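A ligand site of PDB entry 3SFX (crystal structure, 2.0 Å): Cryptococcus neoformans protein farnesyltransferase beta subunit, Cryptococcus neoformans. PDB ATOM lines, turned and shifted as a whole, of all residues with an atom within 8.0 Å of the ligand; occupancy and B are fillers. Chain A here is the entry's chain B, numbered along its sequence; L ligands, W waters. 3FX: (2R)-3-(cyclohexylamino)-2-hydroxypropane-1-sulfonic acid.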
ATOM      1  N   LEU A  50      33.913 -23.856  11.539  1.00  0.00           N
ATOM      2  CA  LEU A  50      34.906 -23.841  10.474  1.00  0.00           C
ATOM      3  C   LEU A  50      35.842 -25.038  10.674  1.00  0.00           C
ATOM      4  O   LEU A  50      36.065 -25.817   9.740  1.00  0.00           O
ATOM      5  CB  LEU A  50      35.714 -22.530  10.474  1.00  0.00           C
ATOM      6  CG  LEU A  50      35.079 -21.183  10.111  1.00  0.00           C
ATOM      7  CD1 LEU A  50      36.092 -20.061  10.352  1.00  0.00           C
ATOM      8  CD2 LEU A  50      34.561 -21.143   8.686  1.00  0.00           C
ATOM      9  N   SER A  52      35.661 -27.958  11.210  1.00  0.00           N
ATOM     10  CA  SER A  52      34.783 -29.132  11.067  1.00  0.00           C
ATOM     11  C   SER A  52      35.475 -30.347  11.667  1.00  0.00           C
ATOM     12  O   SER A  52      36.439 -30.866  11.087  1.00  0.00           O
ATOM     13  CB  SER A  52      34.412 -29.374   9.601  1.00  0.00           C
ATOM     14  OG  SER A  52      33.398 -30.369   9.506  1.00  0.00           O
ATOM     15  N   TYR A  58      29.952 -35.663   9.533  1.00  0.00           N
ATOM     16  CA  TYR A  58      29.674 -34.426   8.816  1.00  0.00           C
ATOM     17  C   TYR A  58      28.170 -34.318   8.510  1.00  0.00           C
ATOM     18  O   TYR A  58      27.588 -35.239   7.931  1.00  0.00           O
ATOM     19  CB  TYR A  58      30.515 -34.325   7.525  1.00  0.00           C
ATOM     20  CG  TYR A  58      30.242 -33.058   6.767  1.00  0.00           C
ATOM     21  CD1 TYR A  58      29.740 -33.085   5.458  1.00  0.00           C
ATOM     22  CD2 TYR A  58      30.447 -31.802   7.364  1.00  0.00           C
ATOM     23  CE1 TYR A  58      29.452 -31.904   4.764  1.00  0.00           C
ATOM     24  CE2 TYR A  58      30.163 -30.615   6.678  1.00  0.00           C
ATOM     25  CZ  TYR A  58      29.661 -30.674   5.379  1.00  0.00           C
ATOM     26  OH  TYR A  58      29.389 -29.498   4.708  1.00  0.00           O
ATOM     27  N   GLY A  60      26.470 -32.214   6.477  1.00  0.00           N
ATOM     28  CA  GLY A  60      26.015 -31.670   5.180  1.00  0.00           C
ATOM     29  C   GLY A  60      24.843 -32.431   4.578  1.00  0.00           C
ATOM     30  O   GLY A  60      24.757 -33.675   4.684  1.00  0.00           O
ATOM     31  N   LEU A  61      23.954 -31.700   3.929  1.00  0.00           N
ATOM     32  CA  LEU A  61      22.767 -32.300   3.314  1.00  0.00           C
ATOM     33  C   LEU A  61      23.190 -33.247   2.194  1.00  0.00           C
ATOM     34  O   LEU A  61      23.835 -32.842   1.225  1.00  0.00           O
ATOM     35  CB  LEU A  61      21.820 -31.211   2.807  1.00  0.00           C
ATOM     36  CG  LEU A  61      20.494 -31.681   2.200  1.00  0.00           C
ATOM     37  CD1 LEU A  61      19.591 -32.271   3.295  1.00  0.00           C
ATOM     38  CD2 LEU A  61      19.802 -30.505   1.480  1.00  0.00           C
ATOM     39  N   ILE A 486      21.521 -20.027   5.576  1.00  0.00           N
ATOM     40  CA  ILE A 486      21.826 -21.413   5.185  1.00  0.00           C
ATOM     41  C   ILE A 486      22.812 -22.017   6.166  1.00  0.00           C
ATOM     42  O   ILE A 486      24.033 -21.823   6.054  1.00  0.00           O
ATOM     43  CB  ILE A 486      22.370 -21.536   3.727  1.00  0.00           C
ATOM     44  CG1 ILE A 486      21.541 -20.662   2.767  1.00  0.00           C
ATOM     45  CG2 ILE A 486      22.403 -23.023   3.279  1.00  0.00           C
ATOM     46  CD1 ILE A 486      20.057 -21.080   2.653  1.00  0.00           C
ATOM     47  N   VAL A 487      22.281 -22.732   7.146  1.00  0.00           N
ATOM     48  CA  VAL A 487      23.118 -23.338   8.177  1.00  0.00           C
ATOM     49  C   VAL A 487      24.050 -24.352   7.501  1.00  0.00           C
ATOM     50  O   VAL A 487      23.605 -25.147   6.669  1.00  0.00           O
ATOM     51  CB  VAL A 487      22.271 -24.010   9.296  1.00  0.00           C
ATOM     52  CG1 VAL A 487      23.131 -24.908  10.205  1.00  0.00           C
ATOM     53  CG2 VAL A 487      21.582 -22.938  10.120  1.00  0.00           C
ATOM     54  N   GLY A 488      25.342 -24.265   7.799  1.00  0.00           N
ATOM     55  CA  GLY A 488      26.322 -25.253   7.312  1.00  0.00           C
ATOM     56  C   GLY A 488      26.969 -24.886   5.986  1.00  0.00           C
ATOM     57  O   GLY A 488      27.859 -25.585   5.520  1.00  0.00           O
ATOM     58  N   GLY A 489      26.519 -23.791   5.389  1.00  0.00           N
ATOM     59  CA  GLY A 489      27.118 -23.287   4.157  1.00  0.00           C
ATOM     60  C   GLY A 489      26.245 -23.525   2.942  1.00  0.00           C
ATOM     61  O   GLY A 489      25.294 -24.325   2.962  1.00  0.00           O
ATOM     62  N   LYS A 490      26.596 -22.848   1.861  1.00  0.00           N
ATOM     63  CA  LYS A 490      25.679 -22.734   0.716  1.00  0.00           C
ATOM     64  C   LYS A 490      25.394 -24.043  -0.018  1.00  0.00           C
ATOM     65  O   LYS A 490      24.383 -24.149  -0.705  1.00  0.00           O
ATOM     66  CB  LYS A 490      26.162 -21.648  -0.250  1.00  0.00           C
ATOM     67  CG  LYS A 490      26.014 -20.242   0.349  1.00  0.00           C
ATOM     68  CD  LYS A 490      26.295 -19.164  -0.687  1.00  0.00           C
ATOM     69  CE  LYS A 490      26.245 -17.768  -0.088  1.00  0.00           C
ATOM     70  NZ  LYS A 490      26.722 -16.779  -1.110  1.00  0.00           N
ATOM     71  N   ASP A 491      26.238 -25.056   0.149  1.00  0.00           N
ATOM     72  CA  ASP A 491      25.937 -26.374  -0.445  1.00  0.00           C
ATOM     73  C   ASP A 491      24.714 -27.025   0.199  1.00  0.00           C
ATOM     74  O   ASP A 491      24.087 -27.921  -0.404  1.00  0.00           O
ATOM     75  CB  ASP A 491      27.146 -27.318  -0.421  1.00  0.00           C
ATOM     76  CG  ASP A 491      28.229 -26.925  -1.408  1.00  0.00           C
ATOM     77  OD1 ASP A 491      27.896 -26.513  -2.536  1.00  0.00           O
ATOM     78  OD2 ASP A 491      29.414 -27.053  -1.076  1.00  0.00           O
ATOM     79  N   ASN A 492      24.341 -26.571   1.402  1.00  0.00           N
ATOM     80  CA  ASN A 492      23.096 -27.058   2.022  1.00  0.00           C
ATOM     81  C   ASN A 492      21.809 -26.394   1.504  1.00  0.00           C
ATOM     82  O   ASN A 492      20.709 -26.832   1.860  1.00  0.00           O
ATOM     83  CB  ASN A 492      23.148 -26.950   3.536  1.00  0.00           C
ATOM     84  CG  ASN A 492      24.156 -27.895   4.159  1.00  0.00           C
ATOM     85  OD1 ASN A 492      24.523 -28.925   3.575  1.00  0.00           O
ATOM     86  ND2 ASN A 492      24.628 -27.532   5.353  1.00  0.00           N
ATOM     87  N   ARG A 493      21.939 -25.357   0.687  1.00  0.00           N
ATOM     88  CA  ARG A 493      20.770 -24.595   0.210  1.00  0.00           C
ATOM     89  C   ARG A 493      19.854 -25.430  -0.669  1.00  0.00           C
ATOM     90  O   ARG A 493      20.306 -26.068  -1.639  1.00  0.00           O
ATOM     91  CB  ARG A 493      21.210 -23.348  -0.574  1.00  0.00           C
ATOM     92  CG  ARG A 493      20.039 -22.457  -1.016  1.00  0.00           C
ATOM     93  CD  ARG A 493      20.373 -21.641  -2.268  1.00  0.00           C
ATOM     94  NE  ARG A 493      19.235 -20.790  -2.654  1.00  0.00           N
ATOM     95  CZ  ARG A 493      18.284 -21.132  -3.539  1.00  0.00           C
ATOM     96  NH1 ARG A 493      18.314 -22.314  -4.162  1.00  0.00           N
ATOM     97  NH2 ARG A 493      17.302 -20.280  -3.798  1.00  0.00           N
HETATM   98  OAA 3FX L   1      30.998 -20.252   1.619  1.00  0.00           O
HETATM   99  OAB 3FX L   1      29.637 -21.202  -0.157  1.00  0.00           O
HETATM  100  OAC 3FX L   1      29.241 -24.210   0.338  1.00  0.00           O
HETATM  101  OAD 3FX L   1      28.952 -21.437   2.184  1.00  0.00           O
HETATM  102  CAE 3FX L   1      32.512 -30.328   0.668  1.00  0.00           C
HETATM  103  CAF 3FX L   1      33.370 -29.055   0.549  1.00  0.00           C
HETATM  104  CAG 3FX L   1      31.490 -30.184   1.827  1.00  0.00           C
HETATM  105  CAH 3FX L   1      32.459 -27.832   0.302  1.00  0.00           C
HETATM  106  CAI 3FX L   1      30.567 -28.982   1.575  1.00  0.00           C
HETATM  107  CAJ 3FX L   1      31.072 -25.346   1.609  1.00  0.00           C
HETATM  108  CAK 3FX L   1      31.071 -22.901   1.492  1.00  0.00           C
HETATM  109  NAL 3FX L   1      30.470 -26.598   1.183  1.00  0.00           N
HETATM  110  CAM 3FX L   1      30.633 -24.167   0.758  1.00  0.00           C
HETATM  111  CAN 3FX L   1      31.396 -27.701   1.450  1.00  0.00           C
HETATM  112  SAO 3FX L   1      30.108 -21.392   1.247  1.00  0.00           S
HETATM  113  O   HOH W   1      28.154 -26.553   2.868  1.00  0.00           O
HETATM  114  O   HOH W   2      31.119 -25.091   4.579  1.00  0.00           O
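Water W1 lies within hydrogen-bond range of O of Gly 488 (2.8 Å) and NAL of the ligand (2.9 Å).
An oxygen (OAD) of the ligand is in hydrogen-bond range of the backbone NH of Lys 490 (2.8 Å).
N of Asp 491 lies within hydrogen-bond range of OAC of the ligand (3.1 Å).
The side-chain carboxylate (OD2) of Asp 491 lies within salt-bridge range of a nitrogen (NAL) of the ligand (2.5 Å).
OH of Tyr 58 touches CAI of the ligand, at 3.4 Å.
Gly 489 touches the ligand.
Hydrophobic or aromatic side chains within 4 Å of the ligand: Tyr 58.
The nearest printed residue that does not touch the ligand is Gly 488 (5.1 Å).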
